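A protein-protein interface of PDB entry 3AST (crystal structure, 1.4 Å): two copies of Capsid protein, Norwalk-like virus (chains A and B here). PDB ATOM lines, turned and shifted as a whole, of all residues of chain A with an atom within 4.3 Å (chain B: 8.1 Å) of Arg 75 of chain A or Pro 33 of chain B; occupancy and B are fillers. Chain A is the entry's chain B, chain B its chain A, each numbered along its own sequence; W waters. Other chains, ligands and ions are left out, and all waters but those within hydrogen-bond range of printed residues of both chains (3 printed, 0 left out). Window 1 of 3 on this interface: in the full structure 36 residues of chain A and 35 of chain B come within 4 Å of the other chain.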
ATOM      1  N   PRO A  33     -25.533 -30.716   8.363  1.00  0.00           N
ATOM      2  CA  PRO A  33     -24.551 -30.237   7.393  1.00  0.00           C
ATOM      3  C   PRO A  33     -23.181 -30.017   8.027  1.00  0.00           C
ATOM      4  O   PRO A  33     -22.992 -29.109   8.842  1.00  0.00           O
ATOM      5  CB  PRO A  33     -25.150 -28.915   6.902  1.00  0.00           C
ATOM      6  CG  PRO A  33     -26.591 -28.984   7.256  1.00  0.00           C
ATOM      7  CD  PRO A  33     -26.637 -29.754   8.529  1.00  0.00           C
ATOM      8  N   SER A  70     -28.808 -30.883   0.909  1.00  0.00           N
ATOM      9  CA  SER A  70     -28.404 -30.330   2.202  1.00  0.00           C
ATOM     10  C   SER A  70     -29.200 -29.090   2.616  1.00  0.00           C
ATOM     11  O   SER A  70     -29.317 -28.795   3.806  1.00  0.00           O
ATOM     12  CB  SER A  70     -26.904 -30.021   2.207  1.00  0.00           C
ATOM     13  OG  SER A  70     -26.552 -29.168   1.134  1.00  0.00           O
ATOM     14  N   GLY A  71     -29.753 -28.373   1.638  1.00  0.00           N
ATOM     15  CA  GLY A  71     -30.490 -27.129   1.903  1.00  0.00           C
ATOM     16  C   GLY A  71     -31.648 -27.256   2.877  1.00  0.00           C
ATOM     17  O   GLY A  71     -31.959 -26.321   3.622  1.00  0.00           O
ATOM     18  N   GLN A  72     -32.277 -28.425   2.879  1.00  0.00           N
ATOM     19  CA  GLN A  72     -33.441 -28.706   3.705  1.00  0.00           C
ATOM     20  C   GLN A  72     -33.046 -29.395   5.016  1.00  0.00           C
ATOM     21  O   GLN A  72     -33.822 -29.430   5.974  1.00  0.00           O
ATOM     22  CB  GLN A  72     -34.369 -29.622   2.921  1.00  0.00           C
ATOM     23  CG  GLN A  72     -35.797 -29.170   2.820  1.00  0.00           C
ATOM     24  CD  GLN A  72     -36.587 -30.043   1.869  1.00  0.00           C
ATOM     25  OE1 GLN A  72     -36.034 -30.614   0.925  1.00  0.00           O
ATOM     26  NE2 GLN A  72     -37.883 -30.165   2.120  1.00  0.00           N
ATOM     27  N   LEU A  73     -31.830 -29.933   5.053  1.00  0.00           N
ATOM     28  CA  LEU A  73     -31.386 -30.780   6.156  1.00  0.00           C
ATOM     29  C   LEU A  73     -31.128 -30.012   7.447  1.00  0.00           C
ATOM     30  O   LEU A  73     -30.428 -28.999   7.443  1.00  0.00           O
ATOM     31  CB  LEU A  73     -30.119 -31.544   5.752  1.00  0.00           C
ATOM     32  CG  LEU A  73     -29.514 -32.507   6.784  1.00  0.00           C
ATOM     33  CD1 LEU A  73     -30.481 -33.630   7.138  1.00  0.00           C
ATOM     34  CD2 LEU A  73     -28.200 -33.080   6.274  1.00  0.00           C
ATOM     35  N   PHE A  74     -31.691 -30.518   8.546  1.00  0.00           N
ATOM     36  CA  PHE A  74     -31.378 -30.034   9.896  1.00  0.00           C
ATOM     37  C   PHE A  74     -31.908 -28.622  10.129  1.00  0.00           C
ATOM     38  O   PHE A  74     -31.277 -27.817  10.807  1.00  0.00           O
ATOM     39  CB  PHE A  74     -29.860 -30.098  10.130  1.00  0.00           C
ATOM     40  CG  PHE A  74     -29.458 -30.241  11.570  1.00  0.00           C
ATOM     41  CD1 PHE A  74     -29.738 -31.402  12.280  1.00  0.00           C
ATOM     42  CD2 PHE A  74     -28.757 -29.222  12.207  1.00  0.00           C
ATOM     43  CE1 PHE A  74     -29.346 -31.539  13.610  1.00  0.00           C
ATOM     44  CE2 PHE A  74     -28.364 -29.349  13.537  1.00  0.00           C
ATOM     45  CZ  PHE A  74     -28.656 -30.515  14.234  1.00  0.00           C
ATOM     46  N   ARG A  75     -33.060 -28.324   9.538  1.00  0.00           N
ATOM     47  CA  ARG A  75     -33.750 -27.060   9.774  1.00  0.00           C
ATOM     48  C   ARG A  75     -35.104 -27.326  10.398  1.00  0.00           C
ATOM     49  O   ARG A  75     -35.695 -28.390  10.199  1.00  0.00           O
ATOM     50  CB  ARG A  75     -33.940 -26.266   8.478  1.00  0.00           C
ATOM     51  CG  ARG A  75     -32.790 -25.348   8.117  1.00  0.00           C
ATOM     52  CD  ARG A  75     -31.706 -26.108   7.399  1.00  0.00           C
ATOM     53  NE  ARG A  75     -30.853 -25.232   6.605  1.00  0.00           N
ATOM     54  CZ  ARG A  75     -29.803 -25.646   5.901  1.00  0.00           C
ATOM     55  NH1 ARG A  75     -29.462 -26.928   5.890  1.00  0.00           N
ATOM     56  NH2 ARG A  75     -29.092 -24.771   5.206  1.00  0.00           N
ATOM     57  N   VAL A  76     -35.573 -26.346  11.162  1.00  0.00           N
ATOM     58  CA  VAL A  76     -36.887 -26.381  11.782  1.00  0.00           C
ATOM     59  C   VAL A  76     -37.598 -25.085  11.415  1.00  0.00           C
ATOM     60  O   VAL A  76     -37.025 -23.998  11.520  1.00  0.00           O
ATOM     61  CB  VAL A  76     -36.776 -26.511  13.321  1.00  0.00           C
ATOM     62  CG1 VAL A  76     -38.147 -26.530  13.974  1.00  0.00           C
ATOM     63  CG2 VAL A  76     -36.009 -27.771  13.695  1.00  0.00           C
ATOM     64  N   VAL A  92     -39.762 -26.777   5.551  1.00  0.00           N
ATOM     65  CA  VAL A  92     -38.701 -25.766   5.577  1.00  0.00           C
ATOM     66  C   VAL A  92     -38.962 -24.595   4.616  1.00  0.00           C
ATOM     67  O   VAL A  92     -38.591 -23.457   4.908  1.00  0.00           O
ATOM     68  CB  VAL A  92     -37.309 -26.415   5.332  1.00  0.00           C
ATOM     69  CG1 VAL A  92     -36.208 -25.362   5.217  1.00  0.00           C
ATOM     70  CG2 VAL A  92     -36.978 -27.394   6.455  1.00  0.00           C
ATOM     71  N   GLY A 107     -36.321 -33.045   6.598  1.00  0.00           N
ATOM     72  CA  GLY A 107     -35.102 -32.435   7.114  1.00  0.00           C
ATOM     73  C   GLY A 107     -35.096 -32.156   8.604  1.00  0.00           C
ATOM     74  O   GLY A 107     -34.081 -31.725   9.142  1.00  0.00           O
ATOM     75  N   PHE A 108     -36.223 -32.393   9.275  1.00  0.00           N
ATOM     76  CA  PHE A 108     -36.331 -32.161  10.716  1.00  0.00           C
ATOM     77  C   PHE A 108     -35.240 -32.964  11.442  1.00  0.00           C
ATOM     78  O   PHE A 108     -34.987 -34.107  11.086  1.00  0.00           O
ATOM     79  CB  PHE A 108     -37.731 -32.571  11.188  1.00  0.00           C
ATOM     80  CG  PHE A 108     -38.047 -32.192  12.612  1.00  0.00           C
ATOM     81  CD1 PHE A 108     -38.541 -30.926  12.925  1.00  0.00           C
ATOM     82  CD2 PHE A 108     -37.881 -33.118  13.640  1.00  0.00           C
ATOM     83  CE1 PHE A 108     -38.844 -30.585  14.250  1.00  0.00           C
ATOM     84  CE2 PHE A 108     -38.188 -32.786  14.961  1.00  0.00           C
ATOM     85  CZ  PHE A 108     -38.664 -31.516  15.263  1.00  0.00           C
ATOM     86  N   PRO A 109     -34.573 -32.361  12.446  1.00  0.00           N
ATOM     87  CA  PRO A 109     -33.477 -33.082  13.110  1.00  0.00           C
ATOM     88  C   PRO A 109     -33.894 -34.410  13.744  1.00  0.00           C
ATOM     89  O   PRO A 109     -35.011 -34.540  14.255  1.00  0.00           O
ATOM     90  CB  PRO A 109     -33.021 -32.097  14.188  1.00  0.00           C
ATOM     91  CG  PRO A 109     -33.370 -30.755  13.634  1.00  0.00           C
ATOM     92  CD  PRO A 109     -34.697 -30.982  12.952  1.00  0.00           C
ATOM     93  N   ILE A 166     -37.739 -19.633  11.501  1.00  0.00           N
ATOM     94  CA  ILE A 166     -36.857 -20.647  10.932  1.00  0.00           C
ATOM     95  C   ILE A 166     -35.550 -20.664  11.714  1.00  0.00           C
ATOM     96  O   ILE A 166     -35.058 -19.626  12.156  1.00  0.00           O
ATOM     97  CB  ILE A 166     -36.575 -20.397   9.418  1.00  0.00           C
ATOM     98  CG1 ILE A 166     -35.627 -21.456   8.840  1.00  0.00           C
ATOM     99  CG2 ILE A 166     -35.969 -19.017   9.183  1.00  0.00           C
ATOM    100  CD1 ILE A 166     -36.274 -22.740   8.452  1.00  0.00           C
ATOM    101  N   GLY A 167     -34.986 -21.851  11.878  1.00  0.00           N
ATOM    102  CA  GLY A 167     -33.685 -21.971  12.495  1.00  0.00           C
ATOM    103  C   GLY A 167     -33.207 -23.396  12.545  1.00  0.00           C
ATOM    104  O   GLY A 167     -33.647 -24.249  11.765  1.00  0.00           O
ATOM    105  N   LEU B  27     -32.776 -27.190  -4.769  1.00  0.00           N
ATOM    106  CA  LEU B  27     -31.341 -26.903  -4.868  1.00  0.00           C
ATOM    107  C   LEU B  27     -30.900 -25.811  -3.899  1.00  0.00           C
ATOM    108  O   LEU B  27     -31.733 -25.087  -3.350  1.00  0.00           O
ATOM    109  CB  LEU B  27     -30.960 -26.546  -6.310  1.00  0.00           C
ATOM    110  CG  LEU B  27     -31.220 -27.638  -7.354  1.00  0.00           C
ATOM    111  CD1 LEU B  27     -30.931 -27.135  -8.756  1.00  0.00           C
ATOM    112  CD2 LEU B  27     -30.412 -28.900  -7.056  1.00  0.00           C
ATOM    113  N   SER B  28     -29.587 -25.694  -3.710  1.00  0.00           N
ATOM    114  CA  SER B  28     -29.012 -24.858  -2.666  1.00  0.00           C
ATOM    115  C   SER B  28     -28.209 -23.675  -3.200  1.00  0.00           C
ATOM    116  O   SER B  28     -27.550 -23.774  -4.235  1.00  0.00           O
ATOM    117  CB  SER B  28     -28.106 -25.704  -1.769  1.00  0.00           C
ATOM    118  OG  SER B  28     -28.798 -26.834  -1.264  1.00  0.00           O
ATOM    119  N   ASN B  29     -28.266 -22.564  -2.473  1.00  0.00           N
ATOM    120  CA  ASN B  29     -27.410 -21.407  -2.714  1.00  0.00           C
ATOM    121  C   ASN B  29     -25.939 -21.799  -2.563  1.00  0.00           C
ATOM    122  O   ASN B  29     -25.605 -22.665  -1.756  1.00  0.00           O
ATOM    123  CB  ASN B  29     -27.786 -20.301  -1.722  1.00  0.00           C
ATOM    124  CG  ASN B  29     -27.357 -18.923  -2.177  1.00  0.00           C
ATOM    125  OD1 ASN B  29     -26.175 -18.587  -2.159  1.00  0.00           O
ATOM    126  ND2 ASN B  29     -28.328 -18.103  -2.560  1.00  0.00           N
ATOM    127  N   SER B  30     -25.065 -21.171  -3.343  1.00  0.00           N
ATOM    128  CA  SER B  30     -23.639 -21.493  -3.297  1.00  0.00           C
ATOM    129  C   SER B  30     -22.801 -20.428  -2.585  1.00  0.00           C
ATOM    130  O   SER B  30     -21.574 -20.543  -2.514  1.00  0.00           O
ATOM    131  CB  SER B  30     -23.109 -21.733  -4.706  1.00  0.00           C
ATOM    132  OG  SER B  30     -23.345 -20.596  -5.512  1.00  0.00           O
ATOM    133  N   ARG B  31     -23.452 -19.391  -2.066  1.00  0.00           N
ATOM    134  CA  ARG B  31     -22.749 -18.420  -1.224  1.00  0.00           C
ATOM    135  C   ARG B  31     -22.996 -18.643   0.268  1.00  0.00           C
ATOM    136  O   ARG B  31     -22.181 -18.253   1.096  1.00  0.00           O
ATOM    137  CB  ARG B  31     -23.051 -16.987  -1.654  1.00  0.00           C
ATOM    138  CG  ARG B  31     -22.313 -16.593  -2.930  1.00  0.00           C
ATOM    139  CD  ARG B  31     -22.703 -15.202  -3.382  1.00  0.00           C
ATOM    140  NE  ARG B  31     -22.024 -14.153  -2.623  1.00  0.00           N
ATOM    141  CZ  ARG B  31     -22.444 -12.897  -2.548  1.00  0.00           C
ATOM    142  NH1 ARG B  31     -23.562 -12.528  -3.160  1.00  0.00           N
ATOM    143  NH2 ARG B  31     -21.750 -12.011  -1.846  1.00  0.00           N
ATOM    144  N   PHE B  32     -24.112 -19.279   0.604  1.00  0.00           N
ATOM    145  CA  PHE B  32     -24.324 -19.799   1.954  1.00  0.00           C
ATOM    146  C   PHE B  32     -25.293 -20.975   1.868  1.00  0.00           C
ATOM    147  O   PHE B  32     -26.076 -21.055   0.924  1.00  0.00           O
ATOM    148  CB  PHE B  32     -24.790 -18.702   2.937  1.00  0.00           C
ATOM    149  CG  PHE B  32     -26.253 -18.370   2.853  1.00  0.00           C
ATOM    150  CD1 PHE B  32     -27.137 -18.850   3.815  1.00  0.00           C
ATOM    151  CD2 PHE B  32     -26.748 -17.572   1.826  1.00  0.00           C
ATOM    152  CE1 PHE B  32     -28.491 -18.539   3.756  1.00  0.00           C
ATOM    153  CE2 PHE B  32     -28.103 -17.265   1.756  1.00  0.00           C
ATOM    154  CZ  PHE B  32     -28.971 -17.744   2.723  1.00  0.00           C
ATOM    155  N   PRO B  33     -25.229 -21.907   2.832  1.00  0.00           N
ATOM    156  CA  PRO B  33     -26.074 -23.092   2.747  1.00  0.00           C
ATOM    157  C   PRO B  33     -27.535 -22.767   3.049  1.00  0.00           C
ATOM    158  O   PRO B  33     -27.881 -22.407   4.178  1.00  0.00           O
ATOM    159  CB  PRO B  33     -25.480 -24.034   3.806  1.00  0.00           C
ATOM    160  CG  PRO B  33     -24.191 -23.404   4.238  1.00  0.00           C
ATOM    161  CD  PRO B  33     -24.348 -21.952   4.010  1.00  0.00           C
ATOM    162  N   SER B  34     -28.373 -22.869   2.021  1.00  0.00           N
ATOM    163  CA  SER B  34     -29.805 -22.606   2.130  1.00  0.00           C
ATOM    164  C   SER B  34     -30.450 -22.981   0.816  1.00  0.00           C
ATOM    165  O   SER B  34     -29.816 -22.892  -0.230  1.00  0.00           O
ATOM    166  CB  SER B  34     -30.059 -21.121   2.396  1.00  0.00           C
ATOM    167  OG  SER B  34     -31.424 -20.770   2.225  1.00  0.00           O
ATOM    168  N   LEU B  35     -31.715 -23.382   0.861  1.00  0.00           N
ATOM    169  CA  LEU B  35     -32.474 -23.612  -0.363  1.00  0.00           C
ATOM    170  C   LEU B  35     -32.577 -22.339  -1.195  1.00  0.00           C
ATOM    171  O   LEU B  35     -32.663 -21.235  -0.655  1.00  0.00           O
ATOM    172  CB  LEU B  35     -33.880 -24.119  -0.044  1.00  0.00           C
ATOM    173  CG  LEU B  35     -34.042 -25.512   0.561  1.00  0.00           C
ATOM    174  CD1 LEU B  35     -35.496 -25.706   0.956  1.00  0.00           C
ATOM    175  CD2 LEU B  35     -33.590 -26.591  -0.414  1.00  0.00           C
ATOM    176  N   ILE B  36     -32.558 -22.515  -2.513  1.00  0.00           N
ATOM    177  CA  ILE B  36     -32.838 -21.434  -3.449  1.00  0.00           C
ATOM    178  C   ILE B  36     -34.323 -21.068  -3.373  1.00  0.00           C
ATOM    179  O   ILE B  36     -35.188 -21.944  -3.361  1.00  0.00           O
ATOM    180  CB  ILE B  36     -32.413 -21.832  -4.881  1.00  0.00           C
ATOM    181  CG1 ILE B  36     -30.879 -21.872  -4.967  1.00  0.00           C
ATOM    182  CG2 ILE B  36     -33.000 -20.868  -5.923  1.00  0.00           C
ATOM    183  CD1 ILE B  36     -30.322 -22.549  -6.208  1.00  0.00           C
ATOM    184  N   THR B  69     -18.198 -28.878  -2.099  1.00  0.00           N
ATOM    185  CA  THR B  69     -19.439 -29.294  -1.449  1.00  0.00           C
ATOM    186  C   THR B  69     -19.877 -28.251  -0.418  1.00  0.00           C
ATOM    187  O   THR B  69     -19.139 -27.307  -0.130  1.00  0.00           O
ATOM    188  CB  THR B  69     -19.254 -30.645  -0.733  1.00  0.00           C
ATOM    189  OG1 THR B  69     -18.132 -30.554   0.152  1.00  0.00           O
ATOM    190  CG2 THR B  69     -19.026 -31.786  -1.727  1.00  0.00           C
ATOM    191  N   SER B  70     -21.063 -28.442   0.154  1.00  0.00           N
ATOM    192  CA  SER B  70     -21.623 -27.499   1.123  1.00  0.00           C
ATOM    193  C   SER B  70     -20.948 -27.550   2.497  1.00  0.00           C
ATOM    194  O   SER B  70     -21.125 -26.645   3.310  1.00  0.00           O
ATOM    195  CB  SER B  70     -23.133 -27.714   1.270  1.00  0.00           C
ATOM    196  OG  SER B  70     -23.823 -27.287   0.109  1.00  0.00           O
ATOM    197  N   GLY B  71     -20.174 -28.607   2.749  1.00  0.00           N
ATOM    198  CA  GLY B  71     -19.522 -28.821   4.051  1.00  0.00           C
ATOM    199  C   GLY B  71     -18.542 -27.759   4.527  1.00  0.00           C
ATOM    200  O   GLY B  71     -18.493 -27.452   5.720  1.00  0.00           O
ATOM    201  N   GLN B  72     -17.740 -27.218   3.611  1.00  0.00           N
ATOM    202  CA  GLN B  72     -16.802 -26.142   3.938  1.00  0.00           C
ATOM    203  C   GLN B  72     -17.427 -24.767   3.768  1.00  0.00           C
ATOM    204  O   GLN B  72     -16.865 -23.770   4.229  1.00  0.00           O
ATOM    205  CB  GLN B  72     -15.574 -26.186   3.030  1.00  0.00           C
ATOM    206  CG  GLN B  72     -14.497 -27.144   3.433  1.00  0.00           C
ATOM    207  CD  GLN B  72     -13.580 -27.451   2.275  1.00  0.00           C
ATOM    208  OE1 GLN B  72     -14.007 -28.004   1.263  1.00  0.00           O
ATOM    209  NE2 GLN B  72     -12.315 -27.076   2.408  1.00  0.00           N
ATOM    210  N   LEU B  73     -18.573 -24.712   3.090  1.00  0.00           N
ATOM    211  CA  LEU B  73     -19.140 -23.436   2.669  1.00  0.00           C
ATOM    212  C   LEU B  73     -19.633 -22.596   3.837  1.00  0.00           C
ATOM    213  O   LEU B  73     -20.407 -23.071   4.671  1.00  0.00           O
ATOM    214  CB  LEU B  73     -20.274 -23.649   1.661  1.00  0.00           C
ATOM    215  CG  LEU B  73     -20.929 -22.376   1.103  1.00  0.00           C
ATOM    216  CD1 LEU B  73     -19.940 -21.524   0.311  1.00  0.00           C
ATOM    217  CD2 LEU B  73     -22.144 -22.719   0.255  1.00  0.00           C
ATOM    218  N   PHE B  74     -19.171 -21.345   3.878  1.00  0.00           N
ATOM    219  CA  PHE B  74     -19.672 -20.342   4.818  1.00  0.00           C
ATOM    220  C   PHE B  74     -19.289 -20.660   6.266  1.00  0.00           C
ATOM    221  O   PHE B  74     -20.049 -20.395   7.194  1.00  0.00           O
ATOM    222  CB  PHE B  74     -21.194 -20.200   4.655  1.00  0.00           C
ATOM    223  CG  PHE B  74     -21.730 -18.844   4.993  1.00  0.00           C
ATOM    224  CD1 PHE B  74     -21.431 -17.740   4.203  1.00  0.00           C
ATOM    225  CD2 PHE B  74     -22.566 -18.677   6.087  1.00  0.00           C
ATOM    226  CE1 PHE B  74     -21.953 -16.481   4.516  1.00  0.00           C
ATOM    227  CE2 PHE B  74     -23.082 -17.434   6.405  1.00  0.00           C
ATOM    228  CZ  PHE B  74     -22.776 -16.335   5.622  1.00  0.00           C
ATOM    229  N   ARG B  75     -18.110 -21.244   6.444  1.00  0.00           N
ATOM    230  CA  ARG B  75     -17.541 -21.478   7.767  1.00  0.00           C
ATOM    231  C   ARG B  75     -16.300 -20.623   7.944  1.00  0.00           C
ATOM    232  O   ARG B  75     -15.615 -20.294   6.972  1.00  0.00           O
ATOM    233  CB  ARG B  75     -17.174 -22.950   7.962  1.00  0.00           C
ATOM    234  CG  ARG B  75     -18.291 -23.836   8.489  1.00  0.00           C
ATOM    235  CD  ARG B  75     -19.236 -24.271   7.393  1.00  0.00           C
ATOM    236  NE  ARG B  75     -20.041 -25.421   7.794  1.00  0.00           N
ATOM    237  CZ  ARG B  75     -20.985 -25.979   7.044  1.00  0.00           C
ATOM    238  NH1 ARG B  75     -21.259 -25.496   5.839  1.00  0.00           N
ATOM    239  NH2 ARG B  75     -21.656 -27.027   7.503  1.00  0.00           N
ATOM    240  N   GLY B 107     -14.194 -21.750   1.383  1.00  0.00           N
ATOM    241  CA  GLY B 107     -15.507 -21.603   2.008  1.00  0.00           C
ATOM    242  C   GLY B 107     -15.717 -20.340   2.823  1.00  0.00           C
ATOM    243  O   GLY B 107     -16.826 -20.080   3.286  1.00  0.00           O
ATOM    244  N   PHE B 111     -19.493 -12.162   1.734  1.00  0.00           N
ATOM    245  CA  PHE B 111     -20.518 -11.130   1.904  1.00  0.00           C
ATOM    246  C   PHE B 111     -19.869  -9.765   2.123  1.00  0.00           C
ATOM    247  O   PHE B 111     -19.384  -9.471   3.217  1.00  0.00           O
ATOM    248  CB  PHE B 111     -21.394 -11.440   3.126  1.00  0.00           C
ATOM    249  CG  PHE B 111     -22.419 -12.533   2.922  1.00  0.00           C
ATOM    250  CD1 PHE B 111     -22.373 -13.416   1.841  1.00  0.00           C
ATOM    251  CD2 PHE B 111     -23.426 -12.694   3.868  1.00  0.00           C
ATOM    252  CE1 PHE B 111     -23.335 -14.424   1.708  1.00  0.00           C
ATOM    253  CE2 PHE B 111     -24.384 -13.687   3.740  1.00  0.00           C
ATOM    254  CZ  PHE B 111     -24.339 -14.557   2.660  1.00  0.00           C
ATOM    255  N   THR B 168     -19.732 -19.441  12.145  1.00  0.00           N
ATOM    256  CA  THR B 168     -20.277 -18.894  10.909  1.00  0.00           C
ATOM    257  C   THR B 168     -20.926 -17.543  11.179  1.00  0.00           C
ATOM    258  O   THR B 168     -21.054 -17.130  12.332  1.00  0.00           O
ATOM    259  CB  THR B 168     -21.311 -19.873  10.285  1.00  0.00           C
ATOM    260  OG1 THR B 168     -21.707 -19.404   8.996  1.00  0.00           O
ATOM    261  CG2 THR B 168     -22.547 -20.024  11.171  1.00  0.00           C
ATOM    262  N   ILE B 169     -21.314 -16.851  10.114  1.00  0.00           N
ATOM    263  CA  ILE B 169     -22.135 -15.654  10.234  1.00  0.00           C
ATOM    264  C   ILE B 169     -23.575 -16.097  10.481  1.00  0.00           C
ATOM    265  O   ILE B 169     -24.118 -16.925   9.741  1.00  0.00           O
ATOM    266  CB  ILE B 169     -22.081 -14.794   8.957  1.00  0.00           C
ATOM    267  CG1 ILE B 169     -20.635 -14.462   8.574  1.00  0.00           C
ATOM    268  CG2 ILE B 169     -22.907 -13.517   9.134  1.00  0.00           C
ATOM    269  CD1 ILE B 169     -20.514 -13.885   7.176  1.00  0.00           C
ATOM    270  N   SER B 219     -31.404 -16.491  -2.055  1.00  0.00           N
ATOM    271  CA  SER B 219     -31.917 -17.031  -0.800  1.00  0.00           C
ATOM    272  C   SER B 219     -31.841 -15.937   0.251  1.00  0.00           C
ATOM    273  O   SER B 219     -30.874 -15.172   0.281  1.00  0.00           O
ATOM    274  CB  SER B 219     -31.088 -18.230  -0.346  1.00  0.00           C
ATOM    275  OG  SER B 219     -30.965 -19.193  -1.377  1.00  0.00           O
ATOM    276  N   ALA B 220     -32.851 -15.866   1.116  1.00  0.00           N
ATOM    277  CA  ALA B 220     -32.886 -14.868   2.181  1.00  0.00           C
ATOM    278  C   ALA B 220     -31.920 -15.222   3.306  1.00  0.00           C
ATOM    279  O   ALA B 220     -31.883 -16.361   3.766  1.00  0.00           O
ATOM    280  CB  ALA B 220     -34.297 -14.728   2.725  1.00  0.00           C
ATOM    281  N   PHE B 221     -31.138 -14.234   3.732  1.00  0.00           N
ATOM    282  CA  PHE B 221     -30.216 -14.385   4.848  1.00  0.00           C
ATOM    283  C   PHE B 221     -30.680 -13.502   6.007  1.00  0.00           C
ATOM    284  O   PHE B 221     -31.058 -12.355   5.775  1.00  0.00           O
ATOM    285  CB  PHE B 221     -28.799 -13.987   4.426  1.00  0.00           C
ATOM    286  CG  PHE B 221     -27.752 -14.410   5.403  1.00  0.00           C
ATOM    287  CD1 PHE B 221     -27.190 -15.676   5.320  1.00  0.00           C
ATOM    288  CD2 PHE B 221     -27.355 -13.563   6.433  1.00  0.00           C
ATOM    289  CE1 PHE B 221     -26.244 -16.094   6.238  1.00  0.00           C
ATOM    290  CE2 PHE B 221     -26.403 -13.972   7.361  1.00  0.00           C
ATOM    291  CZ  PHE B 221     -25.845 -15.240   7.263  1.00  0.00           C
ATOM    292  N   GLN B 239     -25.237 -24.931  -5.594  1.00  0.00           N
ATOM    293  CA  GLN B 239     -24.115 -25.727  -5.098  1.00  0.00           C
ATOM    294  C   GLN B 239     -24.101 -27.147  -5.668  1.00  0.00           C
ATOM    295  O   GLN B 239     -23.032 -27.693  -5.929  1.00  0.00           O
ATOM    296  CB  GLN B 239     -24.070 -25.755  -3.562  1.00  0.00           C
ATOM    297  CG  GLN B 239     -22.807 -26.431  -2.979  1.00  0.00           C
ATOM    298  CD  GLN B 239     -21.516 -25.706  -3.331  1.00  0.00           C
ATOM    299  OE1 GLN B 239     -21.437 -24.480  -3.258  1.00  0.00           O
ATOM    300  NE2 GLN B 239     -20.492 -26.468  -3.702  1.00  0.00           N
HETATM  301  O   HOH W   1     -26.946 -26.523   1.294  1.00  0.00           O
HETATM  302  O   HOH W   2     -32.901 -23.730   3.502  1.00  0.00           O
HETATM  303  O   HOH W   3     -25.207 -28.497  -1.821  1.00  0.00           O
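NH2 of Arg 75 of chain B lies within hydrogen-bond range of O of Pro 33 of chain A (2.8 Å).
O of Pro 33 of chain B sits at hydrogen-bond distance from NH2 of Arg 75 of chain A (2.8 Å).
OG of Ser 70 of chain B is in hydrogen-bond range of OG of Ser 70 of chain A.
The backbone NH (N) of Gly 71 of chain A is in hydrogen-bond range of the side-chain hydroxyl (OG) of Ser 28 of chain B.
The backbone carbonyl oxygen (O) of Ser 70 of chain A sits at hydrogen-bond distance from the guanidinium group (NH1) of Arg 75 of chain A (2.8 Å).
The backbone carbonyl oxygen (O) of Gly 71 of chain B lies close to the guanidinium group (NE) of Arg 75 of chain B (3.3 Å).
The backbone carbonyl oxygen of Gly 71 of chain A sits close to the guanidinium group of Arg 75 of chain A (3.4 Å).
The guanidinium group of Arg 75 of chain A lies within hydrogen-bond range of the backbone carbonyl oxygen of Leu 73 of chain A (2.8 Å).
O of Leu 35 of chain B lies within hydrogen-bond range of OG of Ser 219 of chain B (2.8 Å).
O of Leu 73 of chain B is in hydrogen-bond range of NH1 of Arg 75 of chain B (2.8 Å).
CG of Leu 35 of chain B touches C of Gly 71 of chain A (3.8 Å).
Leu 35 of chain B touches Gln 72 of chain A (CD1 to CG, 3.9 Å).
Arg 75 of chain A touches Ser 34 of chain B (NH2 to N, 3.8 Å).
Of chain B, only Pro 33 and Ser 34 come within 4 Å of Arg 75 of chain A.
Printed residues of chain A within 4 Å of Pro 33 of chain B: Arg 75.
Printed residues of chain A within 4 Å of Leu 35 of chain B: Gly 71 (3.8 Å) and Gln 72 (3.9 Å).
Printed residues of chain B within 4 Å of Gly 71 of chain A: Ser 28 and Leu 35.
Printed residues of chain A within 4 Å of Ser 28 of chain B: Gly 71.
Printed residues of chain B within 4 Å of Pro 33 of chain A: Arg 75.
Val 76 of chain A touches none of the printed residues of chain B.
The nearest residue of chain B that does not touch Arg 75 of chain A is Leu 35 of chain B (5.3 Å).
Of the 25 printed residues of chain B, 6 touch a printed residue of chain A.
Hydrophobic or aromatic side chains of chain B within 4 Å of the printed part of chain A: Pro 33 and Leu 35.
Among the printed residues, 7 pairs touch across the chains.
Pro 33 of chain A touches Arg 75 of chain B, and with the chains exchanged Arg 75 of chain A touches Pro 33 of chain B.
Ser 70 of chain B touches its own counterpart, Ser 70 of chain A.
Positions printed for both chains: 33, 70, 71, 72, 73, 74, 75 and 107.
Of the 7 pairs that touch across the chains among the printed residues, 3 have their exchanged pair printed and touching as well.
Water W3 lies within hydrogen-bond range of the side-chain hydroxyl of Ser 70 of chain B (2.7 Å) and the side-chain hydroxyl of Ser 70 of chain A (3.3 Å).
Water W1 lies within hydrogen-bond range of the side-chain hydroxyl of Ser 70 of chain A, the side-chain hydroxyl of Ser 28 of chain B, the backbone NH of Gly 71 of chain A and the side-chain hydroxyl of Ser 70 of chain B.
Water W2 bridges O of Gly 71 of chain A (2.8 Å) and N of Leu 35 of chain B (2.9 Å).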
